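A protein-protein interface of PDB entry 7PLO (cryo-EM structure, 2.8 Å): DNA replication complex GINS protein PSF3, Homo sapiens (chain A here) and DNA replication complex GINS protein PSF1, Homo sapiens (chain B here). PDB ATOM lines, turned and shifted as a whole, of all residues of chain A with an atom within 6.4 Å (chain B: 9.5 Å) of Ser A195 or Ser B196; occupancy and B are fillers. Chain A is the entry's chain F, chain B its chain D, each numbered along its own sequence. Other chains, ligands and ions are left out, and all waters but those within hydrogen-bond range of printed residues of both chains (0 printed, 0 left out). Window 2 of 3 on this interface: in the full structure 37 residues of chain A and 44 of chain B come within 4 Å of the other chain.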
ATOM      1  N   CYS A 188      19.758   9.241  -9.273  1.00  0.00           N
ATOM      2  CA  CYS A 188      19.604  10.254  -8.236  1.00  0.00           C
ATOM      3  C   CYS A 188      18.818  11.448  -8.754  1.00  0.00           C
ATOM      4  O   CYS A 188      17.981  12.008  -8.033  1.00  0.00           O
ATOM      5  CB  CYS A 188      20.973  10.696  -7.720  1.00  0.00           C
ATOM      6  SG  CYS A 188      21.808   9.469  -6.688  1.00  0.00           S
ATOM      7  N   LYS A 191      15.120  10.385  -8.910  1.00  0.00           N
ATOM      8  CA  LYS A 191      14.553  10.347  -7.567  1.00  0.00           C
ATOM      9  C   LYS A 191      14.618  11.691  -6.848  1.00  0.00           C
ATOM     10  O   LYS A 191      14.133  11.788  -5.717  1.00  0.00           O
ATOM     11  CB  LYS A 191      15.257   9.272  -6.734  1.00  0.00           C
ATOM     12  CG  LYS A 191      14.578   7.920  -6.833  1.00  0.00           C
ATOM     13  CD  LYS A 191      15.409   6.811  -6.216  1.00  0.00           C
ATOM     14  CE  LYS A 191      16.454   6.273  -7.178  1.00  0.00           C
ATOM     15  NZ  LYS A 191      15.868   5.534  -8.336  1.00  0.00           N
ATOM     16  N   GLY A 192      15.194  12.723  -7.465  1.00  0.00           N
ATOM     17  CA  GLY A 192      15.181  14.050  -6.881  1.00  0.00           C
ATOM     18  C   GLY A 192      16.239  14.302  -5.835  1.00  0.00           C
ATOM     19  O   GLY A 192      16.194  15.343  -5.170  1.00  0.00           O
ATOM     20  N   GLN A 193      17.191  13.385  -5.668  1.00  0.00           N
ATOM     21  CA  GLN A 193      18.251  13.532  -4.682  1.00  0.00           C
ATOM     22  C   GLN A 193      19.400  14.409  -5.167  1.00  0.00           C
ATOM     23  O   GLN A 193      20.257  14.777  -4.356  1.00  0.00           O
ATOM     24  CB  GLN A 193      18.768  12.144  -4.300  1.00  0.00           C
ATOM     25  CG  GLN A 193      17.734  11.297  -3.543  1.00  0.00           C
ATOM     26  CD  GLN A 193      17.932   9.798  -3.700  1.00  0.00           C
ATOM     27  OE1 GLN A 193      18.871   9.339  -4.351  1.00  0.00           O
ATOM     28  NE2 GLN A 193      17.033   9.025  -3.101  1.00  0.00           N
ATOM     29  N   ALA A 194      19.438  14.759  -6.455  1.00  0.00           N
ATOM     30  CA  ALA A 194      20.462  15.655  -6.979  1.00  0.00           C
ATOM     31  C   ALA A 194      20.261  17.107  -6.559  1.00  0.00           C
ATOM     32  O   ALA A 194      21.171  17.919  -6.756  1.00  0.00           O
ATOM     33  CB  ALA A 194      20.488  15.571  -8.506  1.00  0.00           C
ATOM     34  N   SER A 195      19.101  17.455  -5.998  1.00  0.00           N
ATOM     35  CA  SER A 195      18.817  18.848  -5.668  1.00  0.00           C
ATOM     36  C   SER A 195      19.571  19.311  -4.428  1.00  0.00           C
ATOM     37  O   SER A 195      19.967  20.479  -4.347  1.00  0.00           O
ATOM     38  CB  SER A 195      17.314  19.031  -5.463  1.00  0.00           C
ATOM     39  OG  SER A 195      16.843  18.228  -4.393  1.00  0.00           O
ATOM     40  N   GLN A 196      19.778  18.423  -3.460  1.00  0.00           N
ATOM     41  CA  GLN A 196      20.272  18.837  -2.155  1.00  0.00           C
ATOM     42  C   GLN A 196      21.730  19.275  -2.219  1.00  0.00           C
ATOM     43  O   GLN A 196      22.551  18.679  -2.920  1.00  0.00           O
ATOM     44  CB  GLN A 196      20.119  17.698  -1.149  1.00  0.00           C
ATOM     45  CG  GLN A 196      20.197  18.135   0.304  1.00  0.00           C
ATOM     46  CD  GLN A 196      20.529  16.990   1.237  1.00  0.00           C
ATOM     47  OE1 GLN A 196      19.837  15.973   1.263  1.00  0.00           O
ATOM     48  NE2 GLN A 196      21.601  17.146   2.006  1.00  0.00           N
ATOM     49  N   ILE A 197      22.038  20.329  -1.469  1.00  0.00           N
ATOM     50  CA  ILE A 197      23.412  20.767  -1.248  1.00  0.00           C
ATOM     51  C   ILE A 197      23.969  19.952  -0.087  1.00  0.00           C
ATOM     52  O   ILE A 197      23.307  19.801   0.946  1.00  0.00           O
ATOM     53  CB  ILE A 197      23.470  22.281  -0.957  1.00  0.00           C
ATOM     54  CG1 ILE A 197      22.718  23.098  -2.030  1.00  0.00           C
ATOM     55  CG2 ILE A 197      24.930  22.768  -0.894  1.00  0.00           C
ATOM     56  CD1 ILE A 197      22.552  24.568  -1.705  1.00  0.00           C
ATOM     57  N   LYS B 141      26.796  24.177  -7.829  1.00  0.00           N
ATOM     58  CA  LYS B 141      25.656  23.406  -8.291  1.00  0.00           C
ATOM     59  C   LYS B 141      24.645  24.387  -8.869  1.00  0.00           C
ATOM     60  O   LYS B 141      24.614  25.541  -8.423  1.00  0.00           O
ATOM     61  CB  LYS B 141      25.057  22.611  -7.121  1.00  0.00           C
ATOM     62  CG  LYS B 141      24.083  21.525  -7.496  1.00  0.00           C
ATOM     63  CD  LYS B 141      23.679  20.653  -6.332  1.00  0.00           C
ATOM     64  CE  LYS B 141      24.774  19.706  -5.908  1.00  0.00           C
ATOM     65  NZ  LYS B 141      24.269  18.622  -5.062  1.00  0.00           N
ATOM     66  N   PRO B 142      23.845  24.010  -9.872  1.00  0.00           N
ATOM     67  CA  PRO B 142      22.940  24.988 -10.485  1.00  0.00           C
ATOM     68  C   PRO B 142      21.915  25.519  -9.496  1.00  0.00           C
ATOM     69  O   PRO B 142      21.417  24.765  -8.646  1.00  0.00           O
ATOM     70  CB  PRO B 142      22.271  24.198 -11.619  1.00  0.00           C
ATOM     71  CG  PRO B 142      22.601  22.816 -11.395  1.00  0.00           C
ATOM     72  CD  PRO B 142      23.889  22.793 -10.702  1.00  0.00           C
ATOM     73  N   PRO B 143      21.570  26.810  -9.565  1.00  0.00           N
ATOM     74  CA  PRO B 143      20.666  27.387  -8.563  1.00  0.00           C
ATOM     75  C   PRO B 143      19.225  26.954  -8.781  1.00  0.00           C
ATOM     76  O   PRO B 143      18.719  27.004  -9.904  1.00  0.00           O
ATOM     77  CB  PRO B 143      20.831  28.891  -8.779  1.00  0.00           C
ATOM     78  CG  PRO B 143      21.173  29.011 -10.196  1.00  0.00           C
ATOM     79  CD  PRO B 143      22.004  27.840 -10.526  1.00  0.00           C
ATOM     80  N   LYS B 144      18.572  26.515  -7.698  1.00  0.00           N
ATOM     81  CA  LYS B 144      17.150  26.186  -7.751  1.00  0.00           C
ATOM     82  C   LYS B 144      16.275  27.251  -7.097  1.00  0.00           C
ATOM     83  O   LYS B 144      15.646  28.042  -7.806  1.00  0.00           O
ATOM     84  CB  LYS B 144      16.929  24.828  -7.079  1.00  0.00           C
ATOM     85  CG  LYS B 144      17.680  23.660  -7.741  1.00  0.00           C
ATOM     86  CD  LYS B 144      17.221  23.351  -9.170  1.00  0.00           C
ATOM     87  CE  LYS B 144      15.805  22.797  -9.211  1.00  0.00           C
ATOM     88  NZ  LYS B 144      15.343  22.539 -10.594  1.00  0.00           N
ATOM     89  N   SER B 145      16.307  27.352  -5.769  1.00  0.00           N
ATOM     90  CA  SER B 145      15.572  28.370  -5.032  1.00  0.00           C
ATOM     91  C   SER B 145      16.539  29.407  -4.488  1.00  0.00           C
ATOM     92  O   SER B 145      17.677  29.101  -4.124  1.00  0.00           O
ATOM     93  CB  SER B 145      14.757  27.768  -3.882  1.00  0.00           C
ATOM     94  OG  SER B 145      15.585  27.076  -2.966  1.00  0.00           O
ATOM     95  N   ILE B 148      16.998  28.955   0.991  1.00  0.00           N
ATOM     96  CA  ILE B 148      16.972  27.571   1.441  1.00  0.00           C
ATOM     97  C   ILE B 148      16.812  27.543   2.951  1.00  0.00           C
ATOM     98  O   ILE B 148      17.194  28.485   3.658  1.00  0.00           O
ATOM     99  CB  ILE B 148      18.240  26.791   1.015  1.00  0.00           C
ATOM    100  CG1 ILE B 148      19.522  27.498   1.478  1.00  0.00           C
ATOM    101  CG2 ILE B 148      18.252  26.605  -0.496  1.00  0.00           C
ATOM    102  CD1 ILE B 148      20.764  26.667   1.297  1.00  0.00           C
ATOM    103  N   GLU B 149      16.251  26.442   3.441  1.00  0.00           N
ATOM    104  CA  GLU B 149      16.142  26.171   4.865  1.00  0.00           C
ATOM    105  C   GLU B 149      17.298  25.276   5.293  1.00  0.00           C
ATOM    106  O   GLU B 149      17.519  24.201   4.709  1.00  0.00           O
ATOM    107  CB  GLU B 149      14.803  25.518   5.195  1.00  0.00           C
ATOM    108  CG  GLU B 149      14.458  25.579   6.660  1.00  0.00           C
ATOM    109  CD  GLU B 149      13.131  24.936   6.975  1.00  0.00           C
ATOM    110  OE1 GLU B 149      12.544  24.293   6.079  1.00  0.00           O
ATOM    111  OE2 GLU B 149      12.674  25.079   8.124  1.00  0.00           O
ATOM    112  N   ARG B 179      20.811  31.068  -0.235  1.00  0.00           N
ATOM    113  CA  ARG B 179      21.659  29.949  -0.622  1.00  0.00           C
ATOM    114  C   ARG B 179      23.109  30.387  -0.785  1.00  0.00           C
ATOM    115  O   ARG B 179      24.033  29.667  -0.382  1.00  0.00           O
ATOM    116  CB  ARG B 179      21.108  29.345  -1.920  1.00  0.00           C
ATOM    117  CG  ARG B 179      21.785  28.059  -2.451  1.00  0.00           C
ATOM    118  CD  ARG B 179      23.069  28.280  -3.278  1.00  0.00           C
ATOM    119  NE  ARG B 179      22.916  29.292  -4.318  1.00  0.00           N
ATOM    120  CZ  ARG B 179      23.910  29.878  -4.974  1.00  0.00           C
ATOM    121  NH1 ARG B 179      25.177  29.565  -4.752  1.00  0.00           N
ATOM    122  NH2 ARG B 179      23.625  30.811  -5.877  1.00  0.00           N
ATOM    123  N   ILE B 186      27.470  24.920   4.426  1.00  0.00           N
ATOM    124  CA  ILE B 186      26.944  23.596   4.095  1.00  0.00           C
ATOM    125  C   ILE B 186      28.064  22.708   3.569  1.00  0.00           C
ATOM    126  O   ILE B 186      28.146  21.519   3.903  1.00  0.00           O
ATOM    127  CB  ILE B 186      25.791  23.697   3.078  1.00  0.00           C
ATOM    128  CG1 ILE B 186      24.595  24.460   3.655  1.00  0.00           C
ATOM    129  CG2 ILE B 186      25.335  22.298   2.663  1.00  0.00           C
ATOM    130  CD1 ILE B 186      23.680  25.030   2.595  1.00  0.00           C
ATOM    131  N   GLU B 192      23.168  22.065   7.342  1.00  0.00           N
ATOM    132  CA  GLU B 192      22.563  21.011   6.535  1.00  0.00           C
ATOM    133  C   GLU B 192      21.365  21.582   5.797  1.00  0.00           C
ATOM    134  O   GLU B 192      20.426  22.068   6.432  1.00  0.00           O
ATOM    135  CB  GLU B 192      22.124  19.836   7.409  1.00  0.00           C
ATOM    136  CG  GLU B 192      21.560  18.660   6.634  1.00  0.00           C
ATOM    137  CD  GLU B 192      21.343  17.444   7.505  1.00  0.00           C
ATOM    138  OE1 GLU B 192      20.593  17.546   8.499  1.00  0.00           O
ATOM    139  OE2 GLU B 192      21.932  16.385   7.202  1.00  0.00           O
ATOM    140  N   HIS B 193      21.394  21.510   4.468  1.00  0.00           N
ATOM    141  CA  HIS B 193      20.240  21.873   3.653  1.00  0.00           C
ATOM    142  C   HIS B 193      19.164  20.807   3.815  1.00  0.00           C
ATOM    143  O   HIS B 193      19.424  19.626   3.564  1.00  0.00           O
ATOM    144  CB  HIS B 193      20.667  22.003   2.193  1.00  0.00           C
ATOM    145  CG  HIS B 193      19.573  22.437   1.269  1.00  0.00           C
ATOM    146  ND1 HIS B 193      19.644  22.257  -0.095  1.00  0.00           N
ATOM    147  CD2 HIS B 193      18.391  23.054   1.503  1.00  0.00           C
ATOM    148  CE1 HIS B 193      18.550  22.736  -0.659  1.00  0.00           C
ATOM    149  NE2 HIS B 193      17.774  23.226   0.289  1.00  0.00           N
ATOM    150  N   ILE B 194      17.954  21.223   4.213  1.00  0.00           N
ATOM    151  CA  ILE B 194      16.945  20.282   4.710  1.00  0.00           C
ATOM    152  C   ILE B 194      15.654  20.334   3.898  1.00  0.00           C
ATOM    153  O   ILE B 194      14.553  20.265   4.459  1.00  0.00           O
ATOM    154  CB  ILE B 194      16.685  20.499   6.216  1.00  0.00           C
ATOM    155  CG1 ILE B 194      16.514  21.984   6.537  1.00  0.00           C
ATOM    156  CG2 ILE B 194      17.829  19.885   7.024  1.00  0.00           C
ATOM    157  CD1 ILE B 194      15.849  22.250   7.872  1.00  0.00           C
ATOM    158  N   LEU B 195      15.766  20.497   2.580  1.00  0.00           N
ATOM    159  CA  LEU B 195      14.671  20.165   1.676  1.00  0.00           C
ATOM    160  C   LEU B 195      15.201  19.354   0.502  1.00  0.00           C
ATOM    161  O   LEU B 195      16.242  19.683  -0.075  1.00  0.00           O
ATOM    162  CB  LEU B 195      13.943  21.416   1.163  1.00  0.00           C
ATOM    163  CG  LEU B 195      12.525  21.182   0.622  1.00  0.00           C
ATOM    164  CD1 LEU B 195      11.546  20.790   1.728  1.00  0.00           C
ATOM    165  CD2 LEU B 195      12.019  22.413  -0.106  1.00  0.00           C
ATOM    166  N   SER B 196      14.473  18.293   0.162  1.00  0.00           N
ATOM    167  CA  SER B 196      14.863  17.371  -0.900  1.00  0.00           C
ATOM    168  C   SER B 196      13.634  16.822  -1.623  1.00  0.00           C
ATOM    169  O   SER B 196      12.576  16.633  -1.021  1.00  0.00           O
ATOM    170  CB  SER B 196      15.686  16.218  -0.327  1.00  0.00           C
ATOM    171  OG  SER B 196      14.943  15.497   0.642  1.00  0.00           O
ATOM    172  OXT SER B 196      13.670  16.547  -2.822  1.00  0.00           O
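Of the 8 printed residues of chain A, 5 touch a printed residue of chain B. Printed residues of chain B that touch a printed residue of chain A: Lys B141, Arg B179, Ile B186, His B193 and Ser B196. Hydrophobic or aromatic side chains of chain B that line the printed part of chain A: Ile B186 and His B193. Among the printed residues, 8 pairs touch across the chains. Among the printed residues, no Asp or Glu carboxylate lies within 4 Å of a Lys or Arg side-chain nitrogen of the other chain.
Lys A191 touches none of the printed residues of chain B. Ala A194 touches just one residue of chain B: Lys B141 (3.6 Å). Ser A195 touches just one residue of chain B: Ser B196. Printed residues of chain B within 4 Å of Gln A196: Lys B141 and His B193. Printed residues of chain B within 4 Å of Ile A197: Arg B179, Ile B186 and His B193. Of the printed residues of chain A, Arg B179 touches Ile A197 (3.7 Å). Of the printed residues of chain A, Ile B186 touches Ile A197 (3.6 Å). Of the printed residues of chain A, His B193 touches Gln A196 and Ile A197. Ile B194 touches none of the printed residues of chain A. Printed residues of chain A within 4 Å of Ser B196: Gly A192 (3.7 Å) and Ser A195 (3.9 Å). The nearest residue of chain B that does not touch Ser A195 is Lys B141 (4.2 Å). The nearest residue of chain A that does not touch Ser B196 is Gln A196 (4.5 Å). The nearest printed residue of chain A that does not touch Arg B179 is Ser A195 (8.0 Å).
O of Gly A192 touches OXT of Ser B196, 3.7 Å away. NZ of Lys B141 touches O of Ala A194 (3.6 Å). OXT of Ser B196 touches OG of Ser A195 (3.9 Å). NE2 of Gln A196 touches O of His B193, at 3.6 Å. CD1 of Ile A197 touches CG of Arg B179, 3.7 Å away. Ile A197 touches Ile B186.
The backbone carbonyl oxygen (O) of Cys A188 sits at hydrogen-bond distance from the backbone NH (N) of Ala A194 (3.5 Å). The backbone carbonyl oxygen of Gly A192 is in hydrogen-bond range of the side-chain hydroxyl of Ser A195 (3.1 Å).
O of Gln A196 sits at hydrogen-bond distance from NZ of Lys B141 (2.7 Å). A ring nitrogen (ND1) of His B193 sits at hydrogen-bond distance from the backbone NH of Ile A197.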
